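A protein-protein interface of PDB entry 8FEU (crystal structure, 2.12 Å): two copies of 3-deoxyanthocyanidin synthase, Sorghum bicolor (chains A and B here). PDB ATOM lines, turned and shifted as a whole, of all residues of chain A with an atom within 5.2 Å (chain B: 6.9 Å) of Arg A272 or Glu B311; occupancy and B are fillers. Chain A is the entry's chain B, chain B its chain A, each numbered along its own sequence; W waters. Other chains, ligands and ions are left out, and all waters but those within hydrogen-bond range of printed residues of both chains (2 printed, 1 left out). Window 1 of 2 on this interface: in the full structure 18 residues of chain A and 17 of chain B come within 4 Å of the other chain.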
ATOM      1  N   VAL A 201      14.966  29.380 -29.264  1.00  0.00           N
ATOM      2  CA  VAL A 201      15.266  28.214 -30.091  1.00  0.00           C
ATOM      3  C   VAL A 201      14.146  27.188 -29.863  1.00  0.00           C
ATOM      4  O   VAL A 201      13.015  27.567 -29.516  1.00  0.00           O
ATOM      5  CB  VAL A 201      16.655  27.653 -29.743  1.00  0.00           C
ATOM      6  CG1 VAL A 201      17.713  28.713 -30.033  1.00  0.00           C
ATOM      7  CG2 VAL A 201      16.722  27.201 -28.272  1.00  0.00           C
ATOM      8  N   LEU A 245      18.089  24.083 -27.718  1.00  0.00           N
ATOM      9  CA  LEU A 245      16.933  23.817 -26.880  1.00  0.00           C
ATOM     10  C   LEU A 245      16.895  24.803 -25.724  1.00  0.00           C
ATOM     11  O   LEU A 245      17.930  25.261 -25.234  1.00  0.00           O
ATOM     12  CB  LEU A 245      16.963  22.386 -26.328  1.00  0.00           C
ATOM     13  CG  LEU A 245      17.289  21.296 -27.344  1.00  0.00           C
ATOM     14  CD1 LEU A 245      17.556  19.945 -26.641  1.00  0.00           C
ATOM     15  CD2 LEU A 245      16.120  21.188 -28.308  1.00  0.00           C
ATOM     16  N   VAL A 246      15.683  25.110 -25.285  1.00  0.00           N
ATOM     17  CA  VAL A 246      15.466  25.863 -24.061  1.00  0.00           C
ATOM     18  C   VAL A 246      14.178  25.348 -23.421  1.00  0.00           C
ATOM     19  O   VAL A 246      13.245  24.931 -24.117  1.00  0.00           O
ATOM     20  CB  VAL A 246      15.435  27.389 -24.335  1.00  0.00           C
ATOM     21  CG1 VAL A 246      14.221  27.779 -25.205  1.00  0.00           C
ATOM     22  CG2 VAL A 246      15.446  28.196 -23.011  1.00  0.00           C
ATOM     23  N   CYS A 270      17.207  33.348 -26.862  1.00  0.00           N
ATOM     24  CA  CYS A 270      16.891  32.562 -25.663  1.00  0.00           C
ATOM     25  C   CYS A 270      17.126  31.087 -25.963  1.00  0.00           C
ATOM     26  O   CYS A 270      16.409  30.491 -26.780  1.00  0.00           O
ATOM     27  CB  CYS A 270      15.458  32.797 -25.190  1.00  0.00           C
ATOM     28  SG  CYS A 270      15.088  32.091 -23.518  1.00  0.00           S
ATOM     29  N   SER A 271      18.112  30.504 -25.287  1.00  0.00           N
ATOM     30  CA  SER A 271      18.657  29.194 -25.618  1.00  0.00           C
ATOM     31  C   SER A 271      19.535  28.757 -24.454  1.00  0.00           C
ATOM     32  O   SER A 271      20.082  29.601 -23.740  1.00  0.00           O
ATOM     33  CB  SER A 271      19.492  29.267 -26.916  1.00  0.00           C
ATOM     34  OG  SER A 271      19.871  27.978 -27.361  1.00  0.00           O
ATOM     35  N   ARG A 272      19.692  27.444 -24.278  1.00  0.00           N
ATOM     36  CA  ARG A 272      20.467  26.975 -23.135  1.00  0.00           C
ATOM     37  C   ARG A 272      21.329  25.759 -23.432  1.00  0.00           C
ATOM     38  O   ARG A 272      22.449  25.671 -22.920  1.00  0.00           O
ATOM     39  CB  ARG A 272      19.554  26.663 -21.943  1.00  0.00           C
ATOM     40  CG  ARG A 272      20.335  26.322 -20.662  1.00  0.00           C
ATOM     41  CD  ARG A 272      21.475  27.343 -20.409  1.00  0.00           C
ATOM     42  NE  ARG A 272      22.327  26.972 -19.282  1.00  0.00           N
ATOM     43  CZ  ARG A 272      23.419  26.216 -19.371  1.00  0.00           C
ATOM     44  NH1 ARG A 272      23.813  25.697 -20.524  1.00  0.00           N
ATOM     45  NH2 ARG A 272      24.147  25.993 -18.278  1.00  0.00           N
ATOM     46  N   TYR A 273      20.823  24.800 -24.211  1.00  0.00           N
ATOM     47  CA  TYR A 273      21.541  23.550 -24.423  1.00  0.00           C
ATOM     48  C   TYR A 273      21.519  23.182 -25.901  1.00  0.00           C
ATOM     49  O   TYR A 273      20.452  23.182 -26.529  1.00  0.00           O
ATOM     50  CB  TYR A 273      20.930  22.405 -23.590  1.00  0.00           C
ATOM     51  CG  TYR A 273      21.916  21.295 -23.361  1.00  0.00           C
ATOM     52  CD1 TYR A 273      22.086  20.293 -24.303  1.00  0.00           C
ATOM     53  CD2 TYR A 273      22.720  21.275 -22.217  1.00  0.00           C
ATOM     54  CE1 TYR A 273      23.024  19.282 -24.117  1.00  0.00           C
ATOM     55  CE2 TYR A 273      23.669  20.258 -22.015  1.00  0.00           C
ATOM     56  CZ  TYR A 273      23.805  19.271 -22.970  1.00  0.00           C
ATOM     57  OH  TYR A 273      24.729  18.279 -22.812  1.00  0.00           O
ATOM     58  N   HIS A 274      22.697  22.849 -26.444  1.00  0.00           N
ATOM     59  CA  HIS A 274      22.915  22.652 -27.881  1.00  0.00           C
ATOM     60  C   HIS A 274      23.519  21.273 -28.124  1.00  0.00           C
ATOM     61  O   HIS A 274      24.723  21.152 -28.389  1.00  0.00           O
ATOM     62  CB  HIS A 274      23.847  23.714 -28.465  1.00  0.00           C
ATOM     63  CG  HIS A 274      23.437  25.120 -28.160  1.00  0.00           C
ATOM     64  ND1 HIS A 274      24.272  26.198 -28.370  1.00  0.00           N
ATOM     65  CD2 HIS A 274      22.289  25.628 -27.647  1.00  0.00           C
ATOM     66  CE1 HIS A 274      23.654  27.310 -28.009  1.00  0.00           C
ATOM     67  NE2 HIS A 274      22.452  26.989 -27.560  1.00  0.00           N
ATOM     68  N   LEU A 310      24.587  32.750 -26.241  1.00  0.00           N
ATOM     69  CA  LEU A 310      23.716  32.807 -25.073  1.00  0.00           C
ATOM     70  C   LEU A 310      23.992  34.020 -24.191  1.00  0.00           C
ATOM     71  O   LEU A 310      23.397  34.145 -23.120  1.00  0.00           O
ATOM     72  CB  LEU A 310      23.863  31.524 -24.245  1.00  0.00           C
ATOM     73  CG  LEU A 310      23.987  30.204 -25.012  1.00  0.00           C
ATOM     74  CD1 LEU A 310      23.936  29.029 -24.058  1.00  0.00           C
ATOM     75  CD2 LEU A 310      22.868  30.081 -26.073  1.00  0.00           C
ATOM     76  N   ILE A 314      22.449  36.641 -20.285  1.00  0.00           N
ATOM     77  CA  ILE A 314      23.317  36.401 -19.130  1.00  0.00           C
ATOM     78  C   ILE A 314      23.968  37.701 -18.677  1.00  0.00           C
ATOM     79  O   ILE A 314      23.950  38.036 -17.486  1.00  0.00           O
ATOM     80  CB  ILE A 314      24.380  35.335 -19.458  1.00  0.00           C
ATOM     81  CG1 ILE A 314      23.732  34.042 -19.958  1.00  0.00           C
ATOM     82  CG2 ILE A 314      25.263  35.073 -18.256  1.00  0.00           C
ATOM     83  CD1 ILE A 314      22.729  33.481 -18.986  1.00  0.00           C
ATOM     84  N   TYR A 320      19.119  30.973 -16.069  1.00  0.00           N
ATOM     85  CA  TYR A 320      18.333  29.815 -16.466  1.00  0.00           C
ATOM     86  C   TYR A 320      18.273  28.804 -15.330  1.00  0.00           C
ATOM     87  O   TYR A 320      19.262  28.585 -14.629  1.00  0.00           O
ATOM     88  CB  TYR A 320      18.950  29.142 -17.691  1.00  0.00           C
ATOM     89  CG  TYR A 320      18.880  29.941 -18.975  1.00  0.00           C
ATOM     90  CD1 TYR A 320      19.776  30.992 -19.221  1.00  0.00           C
ATOM     91  CD2 TYR A 320      17.935  29.639 -19.948  1.00  0.00           C
ATOM     92  CE1 TYR A 320      19.721  31.712 -20.415  1.00  0.00           C
ATOM     93  CE2 TYR A 320      17.876  30.338 -21.140  1.00  0.00           C
ATOM     94  CZ  TYR A 320      18.765  31.379 -21.376  1.00  0.00           C
ATOM     95  OH  TYR A 320      18.676  32.079 -22.572  1.00  0.00           O
ATOM     96  N   HIS A 322      16.976  25.500 -16.035  1.00  0.00           N
ATOM     97  CA  HIS A 322      17.067  24.175 -16.643  1.00  0.00           C
ATOM     98  C   HIS A 322      18.337  24.141 -17.485  1.00  0.00           C
ATOM     99  O   HIS A 322      18.333  24.549 -18.649  1.00  0.00           O
ATOM    100  CB  HIS A 322      15.809  23.872 -17.450  1.00  0.00           C
ATOM    101  CG  HIS A 322      14.550  23.932 -16.647  1.00  0.00           C
ATOM    102  ND1 HIS A 322      13.934  22.805 -16.149  1.00  0.00           N
ATOM    103  CD2 HIS A 322      13.802  24.981 -16.234  1.00  0.00           C
ATOM    104  CE1 HIS A 322      12.848  23.153 -15.485  1.00  0.00           C
ATOM    105  NE2 HIS A 322      12.746  24.468 -15.522  1.00  0.00           N
ATOM    106  N   ASN A 323      19.424  23.653 -16.881  1.00  0.00           N
ATOM    107  CA  ASN A 323      20.757  23.852 -17.415  1.00  0.00           C
ATOM    108  C   ASN A 323      21.389  22.602 -18.007  1.00  0.00           C
ATOM    109  O   ASN A 323      22.299  22.727 -18.835  1.00  0.00           O
ATOM    110  CB  ASN A 323      21.670  24.437 -16.329  1.00  0.00           C
ATOM    111  CG  ASN A 323      21.195  25.806 -15.883  1.00  0.00           C
ATOM    112  OD1 ASN A 323      21.245  26.769 -16.663  1.00  0.00           O
ATOM    113  ND2 ASN A 323      20.684  25.899 -14.649  1.00  0.00           N
ATOM    114  N   ILE A 328      16.190  20.030 -19.033  1.00  0.00           N
ATOM    115  CA  ILE A 328      15.398  20.636 -20.094  1.00  0.00           C
ATOM    116  C   ILE A 328      14.272  19.701 -20.489  1.00  0.00           C
ATOM    117  O   ILE A 328      13.177  20.152 -20.852  1.00  0.00           O
ATOM    118  CB  ILE A 328      16.290  21.012 -21.289  1.00  0.00           C
ATOM    119  CG1 ILE A 328      16.928  22.379 -21.015  1.00  0.00           C
ATOM    120  CG2 ILE A 328      15.450  21.093 -22.576  1.00  0.00           C
ATOM    121  CD1 ILE A 328      18.154  22.683 -21.844  1.00  0.00           C
ATOM    122  N   VAL B 151      26.406  20.814 -14.419  1.00  0.00           N
ATOM    123  CA  VAL B 151      27.104  22.066 -14.686  1.00  0.00           C
ATOM    124  C   VAL B 151      27.808  22.453 -13.387  1.00  0.00           C
ATOM    125  O   VAL B 151      27.168  22.896 -12.438  1.00  0.00           O
ATOM    126  CB  VAL B 151      26.158  23.176 -15.161  1.00  0.00           C
ATOM    127  CG1 VAL B 151      26.979  24.398 -15.626  1.00  0.00           C
ATOM    128  CG2 VAL B 151      25.272  22.670 -16.300  1.00  0.00           C
ATOM    129  N   GLU B 154      31.669  27.902  -9.782  1.00  0.00           N
ATOM    130  CA  GLU B 154      32.731  28.335  -8.895  1.00  0.00           C
ATOM    131  C   GLU B 154      32.508  27.880  -7.448  1.00  0.00           C
ATOM    132  O   GLU B 154      33.446  27.941  -6.648  1.00  0.00           O
ATOM    133  CB  GLU B 154      32.873  29.866  -8.977  1.00  0.00           C
ATOM    134  CG  GLU B 154      33.573  30.373 -10.251  1.00  0.00           C
ATOM    135  CD  GLU B 154      32.616  30.468 -11.454  1.00  0.00           C
ATOM    136  OE1 GLU B 154      31.396  30.232 -11.288  1.00  0.00           O
ATOM    137  OE2 GLU B 154      33.088  30.791 -12.567  1.00  0.00           O
ATOM    138  N   ILE B 269      35.791  30.697 -13.268  1.00  0.00           N
ATOM    139  CA  ILE B 269      36.124  29.764 -14.330  1.00  0.00           C
ATOM    140  C   ILE B 269      36.421  30.551 -15.606  1.00  0.00           C
ATOM    141  O   ILE B 269      35.772  31.559 -15.904  1.00  0.00           O
ATOM    142  CB  ILE B 269      34.972  28.769 -14.531  1.00  0.00           C
ATOM    143  CG1 ILE B 269      34.887  27.818 -13.324  1.00  0.00           C
ATOM    144  CG2 ILE B 269      35.155  27.983 -15.838  1.00  0.00           C
ATOM    145  CD1 ILE B 269      33.544  27.145 -13.211  1.00  0.00           C
ATOM    146  N   THR B 307      30.219  19.575 -17.180  1.00  0.00           N
ATOM    147  CA  THR B 307      30.800  20.708 -17.879  1.00  0.00           C
ATOM    148  C   THR B 307      30.980  21.872 -16.909  1.00  0.00           C
ATOM    149  O   THR B 307      30.414  21.885 -15.818  1.00  0.00           O
ATOM    150  CB  THR B 307      29.904  21.107 -19.092  1.00  0.00           C
ATOM    151  OG1 THR B 307      30.575  22.078 -19.883  1.00  0.00           O
ATOM    152  CG2 THR B 307      28.563  21.686 -18.607  1.00  0.00           C
ATOM    153  N   MET B 308      31.793  22.846 -17.305  1.00  0.00           N
ATOM    154  CA  MET B 308      32.058  24.039 -16.508  1.00  0.00           C
ATOM    155  C   MET B 308      31.142  25.181 -16.928  1.00  0.00           C
ATOM    156  O   MET B 308      30.907  25.394 -18.124  1.00  0.00           O
ATOM    157  CB  MET B 308      33.511  24.473 -16.664  1.00  0.00           C
ATOM    158  CG  MET B 308      34.478  23.339 -16.395  1.00  0.00           C
ATOM    159  SD  MET B 308      34.549  22.958 -14.642  1.00  0.00           S
ATOM    160  CE  MET B 308      36.124  22.108 -14.515  1.00  0.00           C
ATOM    161  N   SER B 309      30.622  25.912 -15.944  1.00  0.00           N
ATOM    162  CA  SER B 309      29.798  27.079 -16.241  1.00  0.00           C
ATOM    163  C   SER B 309      30.678  28.231 -16.697  1.00  0.00           C
ATOM    164  O   SER B 309      31.697  28.527 -16.070  1.00  0.00           O
ATOM    165  CB  SER B 309      28.972  27.511 -15.030  1.00  0.00           C
ATOM    166  OG  SER B 309      28.696  28.902 -15.107  1.00  0.00           O
ATOM    167  N   LEU B 310      30.277  28.882 -17.786  1.00  0.00           N
ATOM    168  CA  LEU B 310      30.984  30.033 -18.325  1.00  0.00           C
ATOM    169  C   LEU B 310      30.389  31.347 -17.853  1.00  0.00           C
ATOM    170  O   LEU B 310      30.806  32.407 -18.327  1.00  0.00           O
ATOM    171  CB  LEU B 310      30.970  30.014 -19.866  1.00  0.00           C
ATOM    172  CG  LEU B 310      31.111  28.659 -20.560  1.00  0.00           C
ATOM    173  CD1 LEU B 310      31.277  28.833 -22.073  1.00  0.00           C
ATOM    174  CD2 LEU B 310      32.279  27.868 -19.984  1.00  0.00           C
ATOM    175  N   GLU B 311      29.414  31.311 -16.953  1.00  0.00           N
ATOM    176  CA  GLU B 311      28.564  32.484 -16.819  1.00  0.00           C
ATOM    177  C   GLU B 311      29.150  33.578 -15.936  1.00  0.00           C
ATOM    178  O   GLU B 311      28.792  34.745 -16.114  1.00  0.00           O
ATOM    179  CB  GLU B 311      27.190  32.058 -16.311  1.00  0.00           C
ATOM    180  CG  GLU B 311      26.569  31.014 -17.233  1.00  0.00           C
ATOM    181  CD  GLU B 311      25.205  30.558 -16.780  1.00  0.00           C
ATOM    182  OE1 GLU B 311      24.645  31.184 -15.855  1.00  0.00           O
ATOM    183  OE2 GLU B 311      24.699  29.560 -17.346  1.00  0.00           O
ATOM    184  N   LYS B 312      30.045  33.261 -15.002  1.00  0.00           N
ATOM    185  CA  LYS B 312      30.424  34.289 -14.037  1.00  0.00           C
ATOM    186  C   LYS B 312      31.152  35.458 -14.710  1.00  0.00           C
ATOM    187  O   LYS B 312      30.747  36.619 -14.555  1.00  0.00           O
ATOM    188  CB  LYS B 312      31.259  33.699 -12.904  1.00  0.00           C
ATOM    189  CG  LYS B 312      31.262  34.637 -11.698  1.00  0.00           C
ATOM    190  CD  LYS B 312      32.169  34.139 -10.568  1.00  0.00           C
ATOM    191  CE  LYS B 312      32.260  35.217  -9.486  1.00  0.00           C
ATOM    192  NZ  LYS B 312      32.966  34.707  -8.264  1.00  0.00           N
ATOM    193  N   LEU B 313      32.226  35.182 -15.456  1.00  0.00           N
ATOM    194  CA  LEU B 313      32.905  36.268 -16.158  1.00  0.00           C
ATOM    195  C   LEU B 313      31.945  37.002 -17.085  1.00  0.00           C
ATOM    196  O   LEU B 313      31.971  38.235 -17.161  1.00  0.00           O
ATOM    197  CB  LEU B 313      34.107  35.745 -16.944  1.00  0.00           C
ATOM    198  CG  LEU B 313      35.419  35.599 -16.171  1.00  0.00           C
ATOM    199  CD1 LEU B 313      36.497  34.954 -17.048  1.00  0.00           C
ATOM    200  CD2 LEU B 313      35.914  36.952 -15.688  1.00  0.00           C
ATOM    201  N   ILE B 314      31.085  36.262 -17.792  1.00  0.00           N
ATOM    202  CA  ILE B 314      30.128  36.892 -18.704  1.00  0.00           C
ATOM    203  C   ILE B 314      29.206  37.823 -17.927  1.00  0.00           C
ATOM    204  O   ILE B 314      28.988  38.980 -18.308  1.00  0.00           O
ATOM    205  CB  ILE B 314      29.324  35.820 -19.465  1.00  0.00           C
ATOM    206  CG1 ILE B 314      30.249  34.903 -20.276  1.00  0.00           C
ATOM    207  CG2 ILE B 314      28.255  36.465 -20.369  1.00  0.00           C
ATOM    208  CD1 ILE B 314      30.957  35.622 -21.396  1.00  0.00           C
ATOM    209  N   ARG B 315      28.636  37.314 -16.832  1.00  0.00           N
ATOM    210  CA  ARG B 315      27.767  38.113 -15.972  1.00  0.00           C
ATOM    211  C   ARG B 315      28.405  39.439 -15.602  1.00  0.00           C
ATOM    212  O   ARG B 315      27.717  40.456 -15.490  1.00  0.00           O
ATOM    213  CB  ARG B 315      27.454  37.337 -14.694  1.00  0.00           C
ATOM    214  CG  ARG B 315      26.027  37.131 -14.431  1.00  0.00           C
ATOM    215  CD  ARG B 315      25.851  36.180 -13.276  1.00  0.00           C
ATOM    216  NE  ARG B 315      25.464  34.860 -13.758  1.00  0.00           N
ATOM    217  CZ  ARG B 315      24.391  34.610 -14.502  1.00  0.00           C
ATOM    218  NH1 ARG B 315      23.596  35.590 -14.939  1.00  0.00           N
ATOM    219  NH2 ARG B 315      24.108  33.347 -14.821  1.00  0.00           N
ATOM    220  N   GLU B 316      29.710  39.443 -15.365  1.00  0.00           N
ATOM    221  CA  GLU B 316      30.367  40.647 -14.874  1.00  0.00           C
ATOM    222  C   GLU B 316      30.869  41.560 -15.986  1.00  0.00           C
ATOM    223  O   GLU B 316      31.490  42.587 -15.690  1.00  0.00           O
ATOM    224  CB  GLU B 316      31.510  40.278 -13.938  1.00  0.00           C
ATOM    225  CG  GLU B 316      31.112  39.154 -12.989  1.00  0.00           C
ATOM    226  CD  GLU B 316      31.673  39.302 -11.599  1.00  0.00           C
ATOM    227  OE1 GLU B 316      32.563  40.150 -11.399  1.00  0.00           O
ATOM    228  OE2 GLU B 316      31.217  38.552 -10.712  1.00  0.00           O
ATOM    229  N   GLY B 317      30.608  41.217 -17.249  1.00  0.00           N
ATOM    230  CA  GLY B 317      30.867  42.105 -18.359  1.00  0.00           C
ATOM    231  C   GLY B 317      32.020  41.704 -19.250  1.00  0.00           C
ATOM    232  O   GLY B 317      32.320  42.428 -20.209  1.00  0.00           O
HETATM  233  O   HOH W   1      21.883  30.886 -16.369  1.00  0.00           O
HETATM  234  O   HOH W   2      24.166  27.142 -15.465  1.00  0.00           O
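Water W1 lies within hydrogen-bond range of N of Tyr A320 (2.8 Å) and OE1 of Glu B311 (2.8 Å).
Water W2 lies within hydrogen-bond range of NH2 of Arg A272 (3.0 Å), OE2 of Glu B311 (3.1 Å) and OD1 of Asn A323 (3.2 Å).
The backbone NH (N) of Arg A272 is in hydrogen-bond range of the backbone carbonyl oxygen (O) of Leu A245 (3.0 Å).
The guanidinium group (NE) of Arg A272 sits at hydrogen-bond distance from the side-chain amide oxygen (OD1) of Asn A323 (2.8 Å).
The side-chain amide nitrogen of Asn A323 lies within hydrogen-bond range of the backbone carbonyl oxygen of Tyr A320 (3.0 Å).
The backbone NH (N) of Glu B311 sits at hydrogen-bond distance from the side-chain hydroxyl (OG) of Ser B309 (3.1 Å).
The side-chain carboxylate of Glu B311 is in salt-bridge range of the guanidinium group of Arg B315 (2.5 Å).
Of the 14 printed residues of chain B, 4 touch a printed residue of chain A.
Printed residues of chain B that touch a printed residue of chain A: Val B151, Glu B311, Ile B314 and Arg B315.
Among the printed residues, 4 pairs touch across the chains.
Of the printed residues of chain B, Asn A323 touches Val B151 (3.9 Å).
Printed residues of chain A within 4 Å of Arg B315: Ile A314.
Printed residues of chain A within 4 Å of Val B151: Asn A323.
Printed residues of chain A within 4 Å of Ile B314: Ile A314.
Leu A245 touches none of the printed residues of chain B.
Met B308 touches none of the printed residues of chain A.
The nearest residue of chain A that does not touch Glu B311 is Ile A314 (4.1 Å).
Ile A314 touches Ile B314.
Arg B315 touches Ile A314.
Asn A323 touches Val B151.
Ile A314 touches its own counterpart, Ile B314.
Positions printed for both chains: 310 and 314.
The guanidinium group (NH2) of Arg A272 lies within salt-bridge range of the side-chain carboxylate (OE2) of Glu B311 (3.7 Å).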
